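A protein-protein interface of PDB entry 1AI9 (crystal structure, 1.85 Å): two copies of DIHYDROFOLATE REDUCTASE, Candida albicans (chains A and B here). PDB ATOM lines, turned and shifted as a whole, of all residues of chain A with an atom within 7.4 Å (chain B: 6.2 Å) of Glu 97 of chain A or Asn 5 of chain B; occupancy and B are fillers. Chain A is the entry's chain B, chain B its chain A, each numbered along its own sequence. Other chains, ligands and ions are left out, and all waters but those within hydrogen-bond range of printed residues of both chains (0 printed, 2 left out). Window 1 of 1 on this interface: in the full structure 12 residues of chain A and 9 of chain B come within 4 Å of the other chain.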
ATOM      1  N   LEU A  77      24.530  15.228 -29.000  1.00  0.00           N
ATOM      2  CA  LEU A  77      24.612  15.487 -27.544  1.00  0.00           C
ATOM      3  C   LEU A  77      23.885  16.733 -27.058  1.00  0.00           C
ATOM      4  O   LEU A  77      24.028  17.759 -27.596  1.00  0.00           O
ATOM      5  CB  LEU A  77      26.148  15.718 -27.234  1.00  0.00           C
ATOM      6  CG  LEU A  77      26.872  14.366 -27.181  1.00  0.00           C
ATOM      7  CD1 LEU A  77      28.317  14.535 -27.570  1.00  0.00           C
ATOM      8  CD2 LEU A  77      26.807  13.861 -25.762  1.00  0.00           C
ATOM      9  N   ASN A  83      19.409   9.228 -22.857  1.00  0.00           N
ATOM     10  CA  ASN A  83      20.026   8.289 -23.882  1.00  0.00           C
ATOM     11  C   ASN A  83      18.827   7.594 -24.558  1.00  0.00           C
ATOM     12  O   ASN A  83      18.071   6.954 -23.828  1.00  0.00           O
ATOM     13  CB  ASN A  83      21.009   7.361 -23.246  1.00  0.00           C
ATOM     14  CG  ASN A  83      22.235   8.055 -22.651  1.00  0.00           C
ATOM     15  OD1 ASN A  83      23.005   7.521 -21.825  1.00  0.00           O
ATOM     16  ND2 ASN A  83      22.510   9.261 -23.091  1.00  0.00           N
ATOM     17  N   ALA A  93      22.233  11.280 -26.859  1.00  0.00           N
ATOM     18  CA  ALA A  93      23.145  10.844 -25.818  1.00  0.00           C
ATOM     19  C   ALA A  93      23.219  12.033 -24.829  1.00  0.00           C
ATOM     20  O   ALA A  93      23.095  13.184 -25.272  1.00  0.00           O
ATOM     21  CB  ALA A  93      24.614  10.632 -26.439  1.00  0.00           C
ATOM     22  N   SER A  94      23.303  11.692 -23.556  1.00  0.00           N
ATOM     23  CA  SER A  94      23.223  12.814 -22.564  1.00  0.00           C
ATOM     24  C   SER A  94      24.515  13.251 -21.979  1.00  0.00           C
ATOM     25  O   SER A  94      24.637  14.267 -21.227  1.00  0.00           O
ATOM     26  CB  SER A  94      22.192  12.460 -21.494  1.00  0.00           C
ATOM     27  OG  SER A  94      22.655  11.484 -20.658  1.00  0.00           O
ATOM     28  N   SER A  95      25.615  12.657 -22.440  1.00  0.00           N
ATOM     29  CA  SER A  95      26.968  13.001 -21.946  1.00  0.00           C
ATOM     30  C   SER A  95      27.954  12.419 -22.909  1.00  0.00           C
ATOM     31  O   SER A  95      27.645  11.502 -23.720  1.00  0.00           O
ATOM     32  CB  SER A  95      27.104  12.343 -20.505  1.00  0.00           C
ATOM     33  OG  SER A  95      27.119  10.941 -20.583  1.00  0.00           O
ATOM     34  N   ILE A  96      29.174  12.973 -22.892  1.00  0.00           N
ATOM     35  CA  ILE A  96      30.185  12.370 -23.808  1.00  0.00           C
ATOM     36  C   ILE A  96      30.422  10.897 -23.485  1.00  0.00           C
ATOM     37  O   ILE A  96      30.658  10.150 -24.394  1.00  0.00           O
ATOM     38  CB  ILE A  96      31.533  13.166 -23.610  1.00  0.00           C
ATOM     39  CG1 ILE A  96      31.276  14.625 -24.108  1.00  0.00           C
ATOM     40  CG2 ILE A  96      32.775  12.526 -24.247  1.00  0.00           C
ATOM     41  CD1 ILE A  96      32.318  15.642 -23.648  1.00  0.00           C
ATOM     42  N   GLU A  97      30.519  10.499 -22.225  1.00  0.00           N
ATOM     43  CA  GLU A  97      30.838   9.141 -21.807  1.00  0.00           C
ATOM     44  C   GLU A  97      29.854   8.122 -22.351  1.00  0.00           C
ATOM     45  O   GLU A  97      30.219   7.058 -22.888  1.00  0.00           O
ATOM     46  CB  GLU A  97      30.933   8.923 -20.295  1.00  0.00           C
ATOM     47  CG  GLU A  97      31.978   9.713 -19.505  1.00  0.00           C
ATOM     48  CD  GLU A  97      31.763  11.186 -19.332  1.00  0.00           C
ATOM     49  OE1 GLU A  97      30.689  11.684 -19.714  1.00  0.00           O
ATOM     50  OE2 GLU A  97      32.714  11.866 -18.922  1.00  0.00           O
ATOM     51  N   SER A  98      28.573   8.595 -22.422  1.00  0.00           N
ATOM     52  CA  SER A  98      27.530   7.738 -23.009  1.00  0.00           C
ATOM     53  C   SER A  98      27.618   7.587 -24.518  1.00  0.00           C
ATOM     54  O   SER A  98      27.367   6.529 -25.089  1.00  0.00           O
ATOM     55  CB  SER A  98      26.148   8.467 -22.726  1.00  0.00           C
ATOM     56  OG  SER A  98      25.820   8.074 -21.435  1.00  0.00           O
ATOM     57  N   SER A  99      27.994   8.675 -25.141  1.00  0.00           N
ATOM     58  CA  SER A  99      28.182   8.772 -26.618  1.00  0.00           C
ATOM     59  C   SER A  99      29.192   7.699 -27.064  1.00  0.00           C
ATOM     60  O   SER A  99      28.959   7.073 -28.067  1.00  0.00           O
ATOM     61  CB  SER A  99      28.492  10.154 -27.116  1.00  0.00           C
ATOM     62  OG  SER A  99      29.720  10.839 -26.887  1.00  0.00           O
ATOM     63  N   LEU A 100      30.276   7.548 -26.312  1.00  0.00           N
ATOM     64  CA  LEU A 100      31.330   6.628 -26.609  1.00  0.00           C
ATOM     65  C   LEU A 100      30.990   5.217 -26.265  1.00  0.00           C
ATOM     66  O   LEU A 100      31.880   4.345 -26.456  1.00  0.00           O
ATOM     67  CB  LEU A 100      32.675   7.201 -26.080  1.00  0.00           C
ATOM     68  CG  LEU A 100      33.185   8.404 -26.896  1.00  0.00           C
ATOM     69  CD1 LEU A 100      34.243   9.221 -26.198  1.00  0.00           C
ATOM     70  CD2 LEU A 100      33.895   7.841 -28.171  1.00  0.00           C
ATOM     71  N   ASN A 101      29.844   5.010 -25.636  1.00  0.00           N
ATOM     72  CA  ASN A 101      29.314   3.707 -25.245  1.00  0.00           C
ATOM     73  C   ASN A 101      28.159   3.308 -26.205  1.00  0.00           C
ATOM     74  O   ASN A 101      27.644   2.183 -26.050  1.00  0.00           O
ATOM     75  CB  ASN A 101      28.819   3.753 -23.762  1.00  0.00           C
ATOM     76  CG  ASN A 101      29.936   3.461 -22.769  1.00  0.00           C
ATOM     77  OD1 ASN A 101      29.817   3.884 -21.595  1.00  0.00           O
ATOM     78  ND2 ASN A 101      30.940   2.691 -23.028  1.00  0.00           N
ATOM     79  N   LEU A 102      27.897   4.139 -27.197  1.00  0.00           N
ATOM     80  CA  LEU A 102      26.846   3.905 -28.177  1.00  0.00           C
ATOM     81  C   LEU A 102      27.360   3.747 -29.623  1.00  0.00           C
ATOM     82  O   LEU A 102      26.520   3.871 -30.539  1.00  0.00           O
ATOM     83  CB  LEU A 102      25.844   5.074 -28.066  1.00  0.00           C
ATOM     84  CG  LEU A 102      24.935   4.968 -26.833  1.00  0.00           C
ATOM     85  CD1 LEU A 102      24.391   6.355 -26.558  1.00  0.00           C
ATOM     86  CD2 LEU A 102      23.791   3.998 -27.170  1.00  0.00           C
ATOM     87  N   ASN A 124      40.634  13.766 -24.240  1.00  0.00           N
ATOM     88  CA  ASN A 124      40.199  12.372 -24.017  1.00  0.00           C
ATOM     89  C   ASN A 124      41.209  11.439 -24.681  1.00  0.00           C
ATOM     90  O   ASN A 124      41.482  11.610 -25.889  1.00  0.00           O
ATOM     91  CB  ASN A 124      38.772  12.191 -24.572  1.00  0.00           C
ATOM     92  CG  ASN A 124      38.122  10.896 -24.106  1.00  0.00           C
ATOM     93  OD1 ASN A 124      36.916  10.992 -23.663  1.00  0.00           O
ATOM     94  ND2 ASN A 124      38.733   9.786 -24.165  1.00  0.00           N
ATOM     95  N   LEU A 126      40.776   8.587 -25.751  1.00  0.00           N
ATOM     96  CA  LEU A 126      40.281   7.822 -26.866  1.00  0.00           C
ATOM     97  C   LEU A 126      40.566   8.468 -28.207  1.00  0.00           C
ATOM     98  O   LEU A 126      40.506   7.678 -29.202  1.00  0.00           O
ATOM     99  CB  LEU A 126      38.810   7.396 -26.694  1.00  0.00           C
ATOM    100  CG  LEU A 126      38.557   6.441 -25.530  1.00  0.00           C
ATOM    101  CD1 LEU A 126      36.999   6.415 -25.328  1.00  0.00           C
ATOM    102  CD2 LEU A 126      39.094   5.034 -25.826  1.00  0.00           C
ATOM    103  N   LYS B   3      22.572   2.727 -21.408  1.00  0.00           N
ATOM    104  CA  LYS B   3      23.955   3.181 -21.207  1.00  0.00           C
ATOM    105  C   LYS B   3      24.156   4.314 -20.256  1.00  0.00           C
ATOM    106  O   LYS B   3      24.761   5.369 -20.561  1.00  0.00           O
ATOM    107  CB  LYS B   3      24.420   3.578 -22.655  1.00  0.00           C
ATOM    108  CG  LYS B   3      24.983   2.627 -23.584  1.00  0.00           C
ATOM    109  CD  LYS B   3      25.235   1.191 -23.396  1.00  0.00           C
ATOM    110  CE  LYS B   3      25.508   0.399 -24.677  1.00  0.00           C
ATOM    111  NZ  LYS B   3      26.124  -0.906 -24.373  1.00  0.00           N
ATOM    112  N   PRO B   4      23.729   4.160 -18.984  1.00  0.00           N
ATOM    113  CA  PRO B   4      23.980   5.169 -17.943  1.00  0.00           C
ATOM    114  C   PRO B   4      25.463   5.213 -17.547  1.00  0.00           C
ATOM    115  O   PRO B   4      26.229   4.264 -17.779  1.00  0.00           O
ATOM    116  CB  PRO B   4      23.134   4.676 -16.775  1.00  0.00           C
ATOM    117  CG  PRO B   4      23.014   3.196 -16.959  1.00  0.00           C
ATOM    118  CD  PRO B   4      23.028   2.944 -18.468  1.00  0.00           C
ATOM    119  N   ASN B   5      25.862   6.335 -16.926  1.00  0.00           N
ATOM    120  CA  ASN B   5      27.294   6.363 -16.418  1.00  0.00           C
ATOM    121  C   ASN B   5      27.210   5.595 -15.110  1.00  0.00           C
ATOM    122  O   ASN B   5      26.017   5.558 -14.586  1.00  0.00           O
ATOM    123  CB  ASN B   5      27.733   7.807 -16.379  1.00  0.00           C
ATOM    124  CG  ASN B   5      27.805   8.367 -17.835  1.00  0.00           C
ATOM    125  OD1 ASN B   5      28.075   7.631 -18.791  1.00  0.00           O
ATOM    126  ND2 ASN B   5      27.302   9.545 -17.998  1.00  0.00           N
ATOM    127  N   VAL B   6      28.147   4.853 -14.677  1.00  0.00           N
ATOM    128  CA  VAL B   6      28.050   4.140 -13.379  1.00  0.00           C
ATOM    129  C   VAL B   6      29.225   4.573 -12.524  1.00  0.00           C
ATOM    130  O   VAL B   6      30.283   4.888 -13.131  1.00  0.00           O
ATOM    131  CB  VAL B   6      27.630   2.707 -13.512  1.00  0.00           C
ATOM    132  CG1 VAL B   6      26.750   2.262 -14.671  1.00  0.00           C
ATOM    133  CG2 VAL B   6      28.455   1.590 -12.966  1.00  0.00           C
ATOM    134  N   ALA B   7      29.092   4.590 -11.195  1.00  0.00           N
ATOM    135  CA  ALA B   7      30.218   4.969 -10.349  1.00  0.00           C
ATOM    136  C   ALA B   7      30.516   3.768  -9.422  1.00  0.00           C
ATOM    137  O   ALA B   7      29.574   2.975  -9.115  1.00  0.00           O
ATOM    138  CB  ALA B   7      29.868   6.269  -9.586  1.00  0.00           C
ATOM    139  N   GLU B 107      18.286   8.051 -11.167  1.00  0.00           N
ATOM    140  CA  GLU B 107      19.229   9.174 -11.419  1.00  0.00           C
ATOM    141  C   GLU B 107      20.647   8.655 -11.547  1.00  0.00           C
ATOM    142  O   GLU B 107      21.202   8.737 -12.680  1.00  0.00           O
ATOM    143  CB  GLU B 107      19.171  10.223 -10.328  1.00  0.00           C
ATOM    144  CG  GLU B 107      19.933  11.515 -10.575  1.00  0.00           C
ATOM    145  CD  GLU B 107      19.639  12.639  -9.649  1.00  0.00           C
ATOM    146  OE1 GLU B 107      18.534  13.170  -9.910  1.00  0.00           O
ATOM    147  OE2 GLU B 107      20.334  13.030  -8.770  1.00  0.00           O
ATOM    148  N   ARG B 108      21.254   8.180 -10.490  1.00  0.00           N
ATOM    149  CA  ARG B 108      22.627   7.654 -10.501  1.00  0.00           C
ATOM    150  C   ARG B 108      22.665   6.191 -10.095  1.00  0.00           C
ATOM    151  O   ARG B 108      21.740   5.692  -9.369  1.00  0.00           O
ATOM    152  CB  ARG B 108      23.566   8.453  -9.605  1.00  0.00           C
ATOM    153  CG  ARG B 108      23.825   9.906 -10.128  1.00  0.00           C
ATOM    154  CD  ARG B 108      24.773  10.512  -9.124  1.00  0.00           C
ATOM    155  NE  ARG B 108      25.379  11.777  -9.532  1.00  0.00           N
ATOM    156  CZ  ARG B 108      25.990  12.596  -8.665  1.00  0.00           C
ATOM    157  NH1 ARG B 108      25.761  12.476  -7.342  1.00  0.00           N
ATOM    158  NH2 ARG B 108      26.756  13.639  -9.050  1.00  0.00           N
ATOM    159  N   VAL B 109      23.706   5.529 -10.571  1.00  0.00           N
ATOM    160  CA  VAL B 109      23.945   4.093 -10.395  1.00  0.00           C
ATOM    161  C   VAL B 109      25.301   3.856  -9.751  1.00  0.00           C
ATOM    162  O   VAL B 109      26.346   4.354 -10.237  1.00  0.00           O
ATOM    163  CB  VAL B 109      23.730   3.392 -11.761  1.00  0.00           C
ATOM    164  CG1 VAL B 109      24.098   1.905 -11.784  1.00  0.00           C
ATOM    165  CG2 VAL B 109      22.318   3.536 -12.310  1.00  0.00           C
ATOM    166  N   SER B 125      33.308  -0.370 -19.725  1.00  0.00           N
ATOM    167  CA  SER B 125      33.284   1.032 -20.128  1.00  0.00           C
ATOM    168  C   SER B 125      32.102   1.818 -19.643  1.00  0.00           C
ATOM    169  O   SER B 125      32.145   3.102 -19.708  1.00  0.00           O
ATOM    170  CB  SER B 125      33.606   1.146 -21.634  1.00  0.00           C
ATOM    171  OG  SER B 125      32.486   0.616 -22.323  1.00  0.00           O
ATOM    172  N   LEU B 126      31.057   1.169 -19.063  1.00  0.00           N
ATOM    173  CA  LEU B 126      29.952   1.964 -18.477  1.00  0.00           C
ATOM    174  C   LEU B 126      30.465   2.673 -17.201  1.00  0.00           C
ATOM    175  O   LEU B 126      29.868   3.789 -16.866  1.00  0.00           O
ATOM    176  CB  LEU B 126      28.760   1.053 -18.162  1.00  0.00           C
ATOM    177  CG  LEU B 126      27.875   0.432 -19.236  1.00  0.00           C
ATOM    178  CD1 LEU B 126      26.769  -0.403 -18.566  1.00  0.00           C
ATOM    179  CD2 LEU B 126      27.156   1.496 -20.035  1.00  0.00           C
ATOM    180  N   VAL B 127      31.469   2.170 -16.573  1.00  0.00           N
ATOM    181  CA  VAL B 127      32.040   2.778 -15.334  1.00  0.00           C
ATOM    182  C   VAL B 127      32.821   4.027 -15.730  1.00  0.00           C
ATOM    183  O   VAL B 127      33.919   3.886 -16.335  1.00  0.00           O
ATOM    184  CB  VAL B 127      32.726   1.803 -14.415  1.00  0.00           C
ATOM    185  CG1 VAL B 127      33.357   2.449 -13.128  1.00  0.00           C
ATOM    186  CG2 VAL B 127      31.826   0.645 -14.062  1.00  0.00           C
ATOM    187  N   SER B 128      32.353   5.176 -15.246  1.00  0.00           N
ATOM    188  CA  SER B 128      32.988   6.445 -15.584  1.00  0.00           C
ATOM    189  C   SER B 128      33.615   7.129 -14.368  1.00  0.00           C
ATOM    190  O   SER B 128      34.500   7.996 -14.599  1.00  0.00           O
ATOM    191  CB  SER B 128      31.945   7.433 -16.205  1.00  0.00           C
ATOM    192  OG  SER B 128      30.913   7.684 -15.290  1.00  0.00           O
ATOM    193  N   HIS B 129      33.171   6.722 -13.189  1.00  0.00           N
ATOM    194  CA  HIS B 129      33.624   7.376 -11.966  1.00  0.00           C
ATOM    195  C   HIS B 129      33.947   6.403 -10.850  1.00  0.00           C
ATOM    196  O   HIS B 129      33.280   5.369 -10.681  1.00  0.00           O
ATOM    197  CB  HIS B 129      32.576   8.422 -11.506  1.00  0.00           C
ATOM    198  CG  HIS B 129      32.236   9.535 -12.417  1.00  0.00           C
ATOM    199  ND1 HIS B 129      31.360   9.396 -13.474  1.00  0.00           N
ATOM    200  CD2 HIS B 129      32.598  10.841 -12.422  1.00  0.00           C
ATOM    201  CE1 HIS B 129      31.178  10.575 -14.046  1.00  0.00           C
ATOM    202  NE2 HIS B 129      31.957  11.467 -13.437  1.00  0.00           N
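1 position is printed for both chains.
Of the 8 pairs that touch across the chains among the printed residues, none has its exchanged pair printed and touching as well.
O of Lys 3 of chain B lies close to OD1 of Asn 83 of chain A (3.1 Å).
ND2 of Asn 5 of chain B sits at hydrogen-bond distance from OG of Ser 95 of chain A.
OG of Ser 125 of chain B is in hydrogen-bond range of ND2 of Asn 101 of chain A (2.7 Å).
The side-chain hydroxyl (OG) of Ser 98 of chain A sits at hydrogen-bond distance from the backbone carbonyl oxygen (O) of Lys 3 of chain B (3.0 Å).
Of the 13 printed residues of chain B, 4 touch a printed residue of chain A.
Printed residues of chain B that touch a printed residue of chain A: Lys 3, Asn 5, Ser 125 and Leu 126.
Among the printed residues, no Asp or Glu carboxylate lies within 4 Å of a Lys or Arg side-chain nitrogen of the other chain.
Printed residues of chain B within 4 Å of Asn 83 of chain A: Lys 3.
Of the printed residues of chain B, Glu 97 of chain A touches Asn 5 (3.5 Å).
Of the printed residues of chain B, Asn 101 of chain A touches Lys 3 (3.1 Å), Ser 125 (2.7 Å) and Leu 126 (3.7 Å).
Asn 5 of chain B touches just these residues of chain A: Ser 95 (2.9 Å), Glu 97 (3.5 Å) and Ser 98 (3.5 Å).
Ala 7 of chain B touches none of the printed residues of chain A.
Printed residues of chain A within 4 Å of Ser 125 of chain B: Asn 101.
The nearest residue of chain A that does not touch Asn 5 of chain B is Asn 101 of chain A (5.0 Å).
ND2 of Asn 83 of chain A lies close to N of Ser 94 of chain A, 2.6 Å away.
OD1 of Asn 101 of chain A sits close to O of Glu 97 of chain A (3.5 Å).
OD1 of Asn 83 of chain A sits at hydrogen-bond distance from OG of Ser 98 of chain A, 2.9 Å away.
O of Leu 126 of chain B is in hydrogen-bond range of N of Val 6 of chain B (3.0 Å).
OG of Ser 95 of chain A lies within hydrogen-bond range of OG of Ser 98 of chain A (3.3 Å).
Among the printed residues, pairs that only touch across the chains: Asn 101 of chain A with Lys 3 of chain B (3.1 Å), Glu 97 of chain A with Asn 5 of chain B (3.5 Å), Ser 98 of chain A with Asn 5 of chain B (3.5 Å) and Asn 101 of chain A with Leu 126 of chain B (3.7 Å).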
